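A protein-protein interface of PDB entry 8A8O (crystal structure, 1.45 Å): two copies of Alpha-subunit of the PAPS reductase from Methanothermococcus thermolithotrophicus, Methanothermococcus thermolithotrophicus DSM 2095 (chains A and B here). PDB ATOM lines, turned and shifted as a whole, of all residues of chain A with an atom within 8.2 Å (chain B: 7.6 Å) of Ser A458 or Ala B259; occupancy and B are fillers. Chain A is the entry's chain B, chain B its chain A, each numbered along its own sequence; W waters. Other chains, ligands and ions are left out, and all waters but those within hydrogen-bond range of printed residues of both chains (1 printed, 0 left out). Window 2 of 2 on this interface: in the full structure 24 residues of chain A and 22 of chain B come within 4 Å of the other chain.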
ATOM      1  N   TYR A 445      24.618  -7.368  19.080  1.00  0.00           N
ATOM      2  CA  TYR A 445      24.152  -6.045  19.442  1.00  0.00           C
ATOM      3  C   TYR A 445      24.929  -5.398  20.572  1.00  0.00           C
ATOM      4  O   TYR A 445      24.639  -4.244  20.912  1.00  0.00           O
ATOM      5  CB  TYR A 445      22.659  -6.081  19.794  1.00  0.00           C
ATOM      6  CG  TYR A 445      21.797  -6.509  18.645  1.00  0.00           C
ATOM      7  CD1 TYR A 445      21.553  -5.647  17.578  1.00  0.00           C
ATOM      8  CD2 TYR A 445      21.222  -7.771  18.612  1.00  0.00           C
ATOM      9  CE1 TYR A 445      20.763  -6.039  16.501  1.00  0.00           C
ATOM     10  CE2 TYR A 445      20.420  -8.169  17.542  1.00  0.00           C
ATOM     11  CZ  TYR A 445      20.199  -7.301  16.489  1.00  0.00           C
ATOM     12  OH  TYR A 445      19.413  -7.691  15.425  1.00  0.00           O
ATOM     13  N   VAL A 455      30.852  -1.314  19.254  1.00  0.00           N
ATOM     14  CA  VAL A 455      29.502  -1.088  19.754  1.00  0.00           C
ATOM     15  C   VAL A 455      29.024   0.287  19.310  1.00  0.00           C
ATOM     16  O   VAL A 455      29.809   1.232  19.187  1.00  0.00           O
ATOM     17  CB  VAL A 455      29.358  -1.250  21.282  1.00  0.00           C
ATOM     18  CG1 VAL A 455      30.053  -2.515  21.756  1.00  0.00           C
ATOM     19  CG2 VAL A 455      29.939  -0.070  22.004  1.00  0.00           C
ATOM     20  N   ASN A 456      27.714   0.407  19.094  1.00  0.00           N
ATOM     21  CA  ASN A 456      27.099   1.705  18.826  1.00  0.00           C
ATOM     22  C   ASN A 456      25.752   1.775  19.530  1.00  0.00           C
ATOM     23  O   ASN A 456      25.170   0.757  19.919  1.00  0.00           O
ATOM     24  CB  ASN A 456      26.998   1.995  17.321  1.00  0.00           C
ATOM     25  CG  ASN A 456      26.111   1.006  16.594  1.00  0.00           C
ATOM     26  OD1 ASN A 456      26.531  -0.118  16.286  1.00  0.00           O
ATOM     27  ND2 ASN A 456      24.894   1.423  16.288  1.00  0.00           N
ATOM     28  N   GLU A 457      25.260   3.000  19.681  1.00  0.00           N
ATOM     29  CA  GLU A 457      24.103   3.241  20.532  1.00  0.00           C
ATOM     30  C   GLU A 457      22.878   2.459  20.070  1.00  0.00           C
ATOM     31  O   GLU A 457      22.199   1.829  20.884  1.00  0.00           O
ATOM     32  CB  GLU A 457      23.807   4.740  20.581  1.00  0.00           C
ATOM     33  CG  GLU A 457      22.618   5.099  21.432  1.00  0.00           C
ATOM     34  CD  GLU A 457      22.939   6.214  22.407  1.00  0.00           C
ATOM     35  OE1 GLU A 457      23.162   7.359  21.955  1.00  0.00           O
ATOM     36  OE2 GLU A 457      22.989   5.938  23.623  1.00  0.00           O
ATOM     37  N   SER A 458      22.573   2.492  18.766  1.00  0.00           N
ATOM     38  CA  SER A 458      21.341   1.865  18.281  1.00  0.00           C
ATOM     39  C   SER A 458      21.312   0.364  18.558  1.00  0.00           C
ATOM     40  O   SER A 458      20.269  -0.192  18.937  1.00  0.00           O
ATOM     41  CB  SER A 458      21.154   2.139  16.789  1.00  0.00           C
ATOM     42  OG  SER A 458      21.032   3.517  16.516  1.00  0.00           O
ATOM     43  N   LYS A 459      22.436  -0.322  18.341  1.00  0.00           N
ATOM     44  CA  LYS A 459      22.491  -1.750  18.617  1.00  0.00           C
ATOM     45  C   LYS A 459      22.417  -2.026  20.114  1.00  0.00           C
ATOM     46  O   LYS A 459      21.724  -2.951  20.539  1.00  0.00           O
ATOM     47  CB  LYS A 459      23.749  -2.343  17.991  1.00  0.00           C
ATOM     48  CG  LYS A 459      23.720  -2.271  16.474  1.00  0.00           C
ATOM     49  CD  LYS A 459      24.773  -3.172  15.852  1.00  0.00           C
ATOM     50  CE  LYS A 459      24.549  -3.294  14.353  1.00  0.00           C
ATOM     51  NZ  LYS A 459      25.698  -3.957  13.689  1.00  0.00           N
ATOM     52  N   LEU A 460      23.082  -1.206  20.933  1.00  0.00           N
ATOM     53  CA  LEU A 460      23.004  -1.384  22.384  1.00  0.00           C
ATOM     54  C   LEU A 460      21.573  -1.232  22.897  1.00  0.00           C
ATOM     55  O   LEU A 460      21.151  -1.961  23.804  1.00  0.00           O
ATOM     56  CB  LEU A 460      23.932  -0.386  23.071  1.00  0.00           C
ATOM     57  CG  LEU A 460      25.413  -0.747  22.958  1.00  0.00           C
ATOM     58  CD1 LEU A 460      26.260   0.418  23.473  1.00  0.00           C
ATOM     59  CD2 LEU A 460      25.756  -2.031  23.718  1.00  0.00           C
ATOM     60  N   LEU A 461      20.819  -0.275  22.358  1.00  0.00           N
ATOM     61  CA  LEU A 461      19.424  -0.125  22.766  1.00  0.00           C
ATOM     62  C   LEU A 461      18.592  -1.346  22.394  1.00  0.00           C
ATOM     63  O   LEU A 461      17.652  -1.701  23.118  1.00  0.00           O
ATOM     64  CB  LEU A 461      18.838   1.109  22.082  1.00  0.00           C
ATOM     65  CG  LEU A 461      19.408   2.434  22.580  1.00  0.00           C
ATOM     66  CD1 LEU A 461      18.814   3.581  21.773  1.00  0.00           C
ATOM     67  CD2 LEU A 461      19.143   2.642  24.058  1.00  0.00           C
ATOM     68  N   ILE A 462      18.905  -1.987  21.270  1.00  0.00           N
ATOM     69  CA  ILE A 462      18.245  -3.230  20.921  1.00  0.00           C
ATOM     70  C   ILE A 462      18.638  -4.325  21.900  1.00  0.00           C
ATOM     71  O   ILE A 462      17.792  -5.126  22.324  1.00  0.00           O
ATOM     72  CB  ILE A 462      18.578  -3.620  19.471  1.00  0.00           C
ATOM     73  CG1 ILE A 462      17.956  -2.631  18.481  1.00  0.00           C
ATOM     74  CG2 ILE A 462      18.087  -5.035  19.162  1.00  0.00           C
ATOM     75  CD1 ILE A 462      18.518  -2.760  17.076  1.00  0.00           C
ATOM     76  N   ALA A 463      19.926  -4.394  22.260  1.00  0.00           N
ATOM     77  CA  ALA A 463      20.373  -5.417  23.201  1.00  0.00           C
ATOM     78  C   ALA A 463      19.644  -5.281  24.531  1.00  0.00           C
ATOM     79  O   ALA A 463      19.234  -6.279  25.133  1.00  0.00           O
ATOM     80  CB  ALA A 463      21.885  -5.321  23.416  1.00  0.00           C
ATOM     81  N   ARG A 464      19.450  -4.048  24.993  1.00  0.00           N
ATOM     82  CA  ARG A 464      18.736  -3.834  26.246  1.00  0.00           C
ATOM     83  C   ARG A 464      17.353  -4.470  26.192  1.00  0.00           C
ATOM     84  O   ARG A 464      16.939  -5.170  27.124  1.00  0.00           O
ATOM     85  CB  ARG A 464      18.629  -2.338  26.519  1.00  0.00           C
ATOM     86  CG  ARG A 464      17.728  -1.979  27.684  1.00  0.00           C
ATOM     87  CD  ARG A 464      17.274  -0.521  27.615  1.00  0.00           C
ATOM     88  NE  ARG A 464      18.255   0.407  28.167  1.00  0.00           N
ATOM     89  CZ  ARG A 464      18.257   1.713  27.941  1.00  0.00           C
ATOM     90  NH1 ARG A 464      17.374   2.273  27.133  1.00  0.00           N
ATOM     91  NH2 ARG A 464      19.152   2.479  28.560  1.00  0.00           N
ATOM     92  N   LEU A 506      26.266   1.616  27.111  1.00  0.00           N
ATOM     93  CA  LEU A 506      25.437   2.719  26.634  1.00  0.00           C
ATOM     94  C   LEU A 506      25.859   4.037  27.269  1.00  0.00           C
ATOM     95  O   LEU A 506      25.808   5.097  26.630  1.00  0.00           O
ATOM     96  CB  LEU A 506      23.978   2.451  26.980  1.00  0.00           C
ATOM     97  CG  LEU A 506      23.151   1.626  26.001  1.00  0.00           C
ATOM     98  CD1 LEU A 506      21.860   1.173  26.662  1.00  0.00           C
ATOM     99  CD2 LEU A 506      22.876   2.444  24.745  1.00  0.00           C
ATOM    100  N   ARG A 519      33.566   2.143  21.423  1.00  0.00           N
ATOM    101  CA  ARG A 519      32.356   2.913  21.123  1.00  0.00           C
ATOM    102  C   ARG A 519      32.576   3.631  19.800  1.00  0.00           C
ATOM    103  O   ARG A 519      33.022   4.780  19.764  1.00  0.00           O
ATOM    104  CB  ARG A 519      32.091   3.915  22.240  1.00  0.00           C
ATOM    105  CG  ARG A 519      30.678   4.472  22.332  1.00  0.00           C
ATOM    106  CD  ARG A 519      29.611   3.403  22.305  1.00  0.00           C
ATOM    107  NE  ARG A 519      28.708   3.596  23.433  1.00  0.00           N
ATOM    108  CZ  ARG A 519      27.602   4.327  23.393  1.00  0.00           C
ATOM    109  NH1 ARG A 519      27.186   4.887  22.270  1.00  0.00           N
ATOM    110  NH2 ARG A 519      26.895   4.495  24.506  1.00  0.00           N
ATOM    111  N   ASP A 521      30.726   5.079  17.754  1.00  0.00           N
ATOM    112  CA  ASP A 521      30.031   6.346  17.546  1.00  0.00           C
ATOM    113  C   ASP A 521      30.595   7.484  18.395  1.00  0.00           C
ATOM    114  O   ASP A 521      30.256   8.646  18.144  1.00  0.00           O
ATOM    115  CB  ASP A 521      28.512   6.211  17.746  1.00  0.00           C
ATOM    116  CG  ASP A 521      28.125   5.310  18.913  1.00  0.00           C
ATOM    117  OD1 ASP A 521      29.003   4.661  19.521  1.00  0.00           O
ATOM    118  OD2 ASP A 521      26.917   5.268  19.219  1.00  0.00           O
ATOM    119  N   ILE B 257      17.239   2.223   5.096  1.00  0.00           N
ATOM    120  CA  ILE B 257      17.694   3.234   6.037  1.00  0.00           C
ATOM    121  C   ILE B 257      18.650   2.605   7.039  1.00  0.00           C
ATOM    122  O   ILE B 257      18.582   1.407   7.327  1.00  0.00           O
ATOM    123  CB  ILE B 257      16.514   3.914   6.779  1.00  0.00           C
ATOM    124  CG1 ILE B 257      15.681   2.863   7.523  1.00  0.00           C
ATOM    125  CG2 ILE B 257      15.655   4.728   5.823  1.00  0.00           C
ATOM    126  CD1 ILE B 257      14.880   3.440   8.670  1.00  0.00           C
ATOM    127  N   ASN B 258      19.545   3.428   7.585  1.00  0.00           N
ATOM    128  CA  ASN B 258      20.373   2.991   8.700  1.00  0.00           C
ATOM    129  C   ASN B 258      19.630   3.271  10.006  1.00  0.00           C
ATOM    130  O   ASN B 258      18.474   3.704  10.009  1.00  0.00           O
ATOM    131  CB  ASN B 258      21.762   3.621   8.642  1.00  0.00           C
ATOM    132  CG  ASN B 258      21.737   5.119   8.765  1.00  0.00           C
ATOM    133  OD1 ASN B 258      20.762   5.715   9.248  1.00  0.00           O
ATOM    134  ND2 ASN B 258      22.828   5.759   8.341  1.00  0.00           N
ATOM    135  N   ALA B 259      20.291   3.011  11.136  1.00  0.00           N
ATOM    136  CA  ALA B 259      19.626   3.159  12.426  1.00  0.00           C
ATOM    137  C   ALA B 259      19.406   4.621  12.778  1.00  0.00           C
ATOM    138  O   ALA B 259      18.609   4.918  13.673  1.00  0.00           O
ATOM    139  CB  ALA B 259      20.435   2.480  13.532  1.00  0.00           C
ATOM    140  N   LEU B 260      20.116   5.529  12.111  1.00  0.00           N
ATOM    141  CA  LEU B 260      19.878   6.957  12.234  1.00  0.00           C
ATOM    142  C   LEU B 260      18.725   7.429  11.357  1.00  0.00           C
ATOM    143  O   LEU B 260      18.366   8.605  11.418  1.00  0.00           O
ATOM    144  CB  LEU B 260      21.151   7.724  11.869  1.00  0.00           C
ATOM    145  CG  LEU B 260      22.444   7.273  12.548  1.00  0.00           C
ATOM    146  CD1 LEU B 260      23.601   8.185  12.169  1.00  0.00           C
ATOM    147  CD2 LEU B 260      22.285   7.223  14.058  1.00  0.00           C
ATOM    148  N   GLY B 261      18.120   6.547  10.572  1.00  0.00           N
ATOM    149  CA  GLY B 261      17.058   6.938   9.677  1.00  0.00           C
ATOM    150  C   GLY B 261      17.501   7.533   8.364  1.00  0.00           C
ATOM    151  O   GLY B 261      16.658   8.057   7.631  1.00  0.00           O
ATOM    152  N   GLU B 262      18.790   7.479   8.039  1.00  0.00           N
ATOM    153  CA  GLU B 262      19.289   8.065   6.804  1.00  0.00           C
ATOM    154  C   GLU B 262      19.167   7.069   5.658  1.00  0.00           C
ATOM    155  O   GLU B 262      19.452   5.878   5.820  1.00  0.00           O
ATOM    156  CB  GLU B 262      20.749   8.500   6.950  1.00  0.00           C
ATOM    157  CG  GLU B 262      21.005   9.461   8.101  1.00  0.00           C
ATOM    158  CD  GLU B 262      22.436   9.421   8.625  1.00  0.00           C
ATOM    159  OE1 GLU B 262      23.278   8.668   8.085  1.00  0.00           O
ATOM    160  OE2 GLU B 262      22.723  10.170   9.582  1.00  0.00           O
ATOM    161  N   TYR B 264      20.857   5.728   3.139  1.00  0.00           N
ATOM    162  CA  TYR B 264      22.284   5.729   2.843  1.00  0.00           C
ATOM    163  C   TYR B 264      22.589   5.422   1.387  1.00  0.00           C
ATOM    164  O   TYR B 264      23.685   5.754   0.925  1.00  0.00           O
ATOM    165  CB  TYR B 264      23.016   4.768   3.797  1.00  0.00           C
ATOM    166  CG  TYR B 264      22.483   3.359   3.795  1.00  0.00           C
ATOM    167  CD1 TYR B 264      21.464   2.995   4.659  1.00  0.00           C
ATOM    168  CD2 TYR B 264      23.012   2.384   2.961  1.00  0.00           C
ATOM    169  CE1 TYR B 264      20.967   1.726   4.671  1.00  0.00           C
ATOM    170  CE2 TYR B 264      22.517   1.106   2.970  1.00  0.00           C
ATOM    171  CZ  TYR B 264      21.497   0.777   3.840  1.00  0.00           C
ATOM    172  OH  TYR B 264      20.976  -0.495   3.892  1.00  0.00           O
ATOM    173  N   GLU B 283      27.572   0.635   6.430  1.00  0.00           N
ATOM    174  CA  GLU B 283      26.819   1.296   7.491  1.00  0.00           C
ATOM    175  C   GLU B 283      27.030   0.579   8.816  1.00  0.00           C
ATOM    176  O   GLU B 283      27.266   1.210   9.858  1.00  0.00           O
ATOM    177  CB  GLU B 283      25.333   1.344   7.130  1.00  0.00           C
ATOM    178  CG  GLU B 283      24.979   2.337   6.028  1.00  0.00           C
ATOM    179  CD  GLU B 283      25.458   3.757   6.319  1.00  0.00           C
ATOM    180  OE1 GLU B 283      25.031   4.335   7.341  1.00  0.00           O
ATOM    181  OE2 GLU B 283      26.264   4.298   5.524  1.00  0.00           O
ATOM    182  N   GLY B 287      29.347   1.852  12.373  1.00  0.00           N
ATOM    183  CA  GLY B 287      28.642   2.180  13.589  1.00  0.00           C
ATOM    184  C   GLY B 287      27.319   2.872  13.403  1.00  0.00           C
ATOM    185  O   GLY B 287      26.876   3.580  14.315  1.00  0.00           O
ATOM    186  N   ARG B 288      26.671   2.689  12.257  1.00  0.00           N
ATOM    187  CA  ARG B 288      25.369   3.283  11.994  1.00  0.00           C
ATOM    188  C   ARG B 288      24.291   2.232  11.781  1.00  0.00           C
ATOM    189  O   ARG B 288      23.179   2.578  11.365  1.00  0.00           O
ATOM    190  CB  ARG B 288      25.451   4.227  10.790  1.00  0.00           C
ATOM    191  CG  ARG B 288      26.291   5.482  11.059  1.00  0.00           C
ATOM    192  CD  ARG B 288      26.282   6.437   9.870  1.00  0.00           C
ATOM    193  NE  ARG B 288      26.844   5.789   8.693  1.00  0.00           N
ATOM    194  CZ  ARG B 288      28.132   5.763   8.391  1.00  0.00           C
ATOM    195  NH1 ARG B 288      29.026   6.422   9.113  1.00  0.00           N
ATOM    196  NH2 ARG B 288      28.537   5.062   7.339  1.00  0.00           N
ATOM    197  N   GLY B 289      24.580   0.964  12.061  1.00  0.00           N
ATOM    198  CA  GLY B 289      23.601  -0.087  11.936  1.00  0.00           C
ATOM    199  C   GLY B 289      22.741  -0.231  13.175  1.00  0.00           C
ATOM    200  O   GLY B 289      22.955   0.435  14.191  1.00  0.00           O
ATOM    201  N   PRO B 290      21.740  -1.112  13.111  1.00  0.00           N
ATOM    202  CA  PRO B 290      21.450  -1.959  11.954  1.00  0.00           C
ATOM    203  C   PRO B 290      20.863  -1.182  10.785  1.00  0.00           C
ATOM    204  O   PRO B 290      20.557   0.007  10.923  1.00  0.00           O
ATOM    205  CB  PRO B 290      20.386  -2.938  12.486  1.00  0.00           C
ATOM    206  CG  PRO B 290      20.347  -2.712  13.987  1.00  0.00           C
ATOM    207  CD  PRO B 290      20.745  -1.298  14.181  1.00  0.00           C
ATOM    208  N   CYS B 291      20.714  -1.848   9.648  1.00  0.00           N
ATOM    209  CA  CYS B 291      20.030  -1.290   8.495  1.00  0.00           C
ATOM    210  C   CYS B 291      18.682  -1.975   8.316  1.00  0.00           C
ATOM    211  O   CYS B 291      18.490  -3.138   8.704  1.00  0.00           O
ATOM    212  CB  CYS B 291      20.869  -1.478   7.234  1.00  0.00           C
ATOM    213  SG  CYS B 291      22.346  -0.444   7.255  1.00  0.00           S
ATOM    214  N   TYR B 292      17.760  -1.246   7.700  1.00  0.00           N
ATOM    215  CA  TYR B 292      16.384  -1.682   7.654  1.00  0.00           C
ATOM    216  C   TYR B 292      15.740  -1.270   6.341  1.00  0.00           C
ATOM    217  O   TYR B 292      16.220  -0.373   5.644  1.00  0.00           O
ATOM    218  CB  TYR B 292      15.526  -0.997   8.725  1.00  0.00           C
ATOM    219  CG  TYR B 292      15.950  -1.154  10.155  1.00  0.00           C
ATOM    220  CD1 TYR B 292      16.873  -0.300  10.731  1.00  0.00           C
ATOM    221  CD2 TYR B 292      15.382  -2.143  10.946  1.00  0.00           C
ATOM    222  CE1 TYR B 292      17.240  -0.438  12.070  1.00  0.00           C
ATOM    223  CE2 TYR B 292      15.738  -2.291  12.268  1.00  0.00           C
ATOM    224  CZ  TYR B 292      16.675  -1.445  12.826  1.00  0.00           C
ATOM    225  OH  TYR B 292      17.025  -1.591  14.150  1.00  0.00           O
ATOM    226  N   ARG B 296       7.813   2.027   8.147  1.00  0.00           N
ATOM    227  CA  ARG B 296       7.067   2.881   9.060  1.00  0.00           C
ATOM    228  C   ARG B 296       6.080   3.749   8.288  1.00  0.00           C
ATOM    229  O   ARG B 296       6.432   4.381   7.286  1.00  0.00           O
ATOM    230  CB  ARG B 296       8.046   3.749   9.850  1.00  0.00           C
ATOM    231  CG  ARG B 296       8.808   2.997  10.927  1.00  0.00           C
ATOM    232  CD  ARG B 296       9.914   3.847  11.539  1.00  0.00           C
ATOM    233  NE  ARG B 296      10.704   4.565  10.545  1.00  0.00           N
ATOM    234  CZ  ARG B 296      11.648   5.448  10.844  1.00  0.00           C
ATOM    235  NH1 ARG B 296      11.942   5.746  12.098  1.00  0.00           N
ATOM    236  NH2 ARG B 296      12.308   6.054   9.859  1.00  0.00           N
ATOM    237  N   PRO B 332      10.672  -0.616  11.506  1.00  0.00           N
ATOM    238  CA  PRO B 332      11.208  -1.040  10.205  1.00  0.00           C
ATOM    239  C   PRO B 332      11.796  -2.444  10.292  1.00  0.00           C
ATOM    240  O   PRO B 332      12.016  -2.988  11.377  1.00  0.00           O
ATOM    241  CB  PRO B 332      12.286   0.005   9.906  1.00  0.00           C
ATOM    242  CG  PRO B 332      12.746   0.437  11.244  1.00  0.00           C
ATOM    243  CD  PRO B 332      11.533   0.401  12.152  1.00  0.00           C
HETATM  244  O   HOH W   1      26.690  -0.596  13.302  1.00  0.00           O
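The backbone carbonyl oxygen of Gly B289 lies within hydrogen-bond range of the side-chain amide nitrogen of Asn A456 (3.0 Å).
N of Tyr B292 lies within hydrogen-bond range of O of Ile B257 (2.8 Å).
The backbone NH (N) of Ala B259 sits at hydrogen-bond distance from the backbone carbonyl oxygen (O) of Arg B288 (2.9 Å).
The backbone carbonyl oxygen (O) of Pro B290 lies within hydrogen-bond range of the backbone NH (N) of Ala B259 (3.0 Å).
O of Glu B283 sits at hydrogen-bond distance from N of Gly B289 (3.5 Å).
Among the printed residues, pairs that only touch across the chains: Asn A456 with Gly B287 (3.4 Å), Ser A458 with Ala B259 (3.2 Å), Ser A458 with Gly B289 (3.6 Å), Lys A459 with Gly B289 (3.6 Å), Lys A459 with Pro B290 (3.8 Å), Ile A462 with Pro B290 (3.6 Å) and Ile A462 with Tyr B292 (3.5 Å).
Of chain B, only Ala B259 (3.2 Å) and Gly B289 (3.6 Å) come within 4 Å of Ser A458.
Ala B259 touches just one residue of chain A: Ser A458.
Printed residues of chain A within 4 Å of Tyr B292: Ile A462 (3.5 Å).
Of the printed residues of chain B, Asn A456 touches Gly B287 and Gly B289.
The nearest printed residue of chain B that does not touch Asn A456 is Arg B288 (4.6 Å).
Printed residues of chain B that touch a printed residue of chain A: Ala B259, Gly B287, Gly B289, Pro B290 and Tyr B292.
Hydrophobic or aromatic side chains of chain A that line the printed part of chain B: Ile A462.
Among the printed residues, 8 pairs touch across the chains.
Among the printed residues, no Asp or Glu carboxylate lies within 4 Å of a Lys or Arg side-chain nitrogen of the other chain.
No position is printed for both chains.
Water W1 lies within hydrogen-bond range of the backbone NH (N) of Gly B289 (2.9 Å), the side-chain amide oxygen (OD1) of Asn A456 (3.0 Å) and the backbone NH (N) of Arg B288 (3.4 Å).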
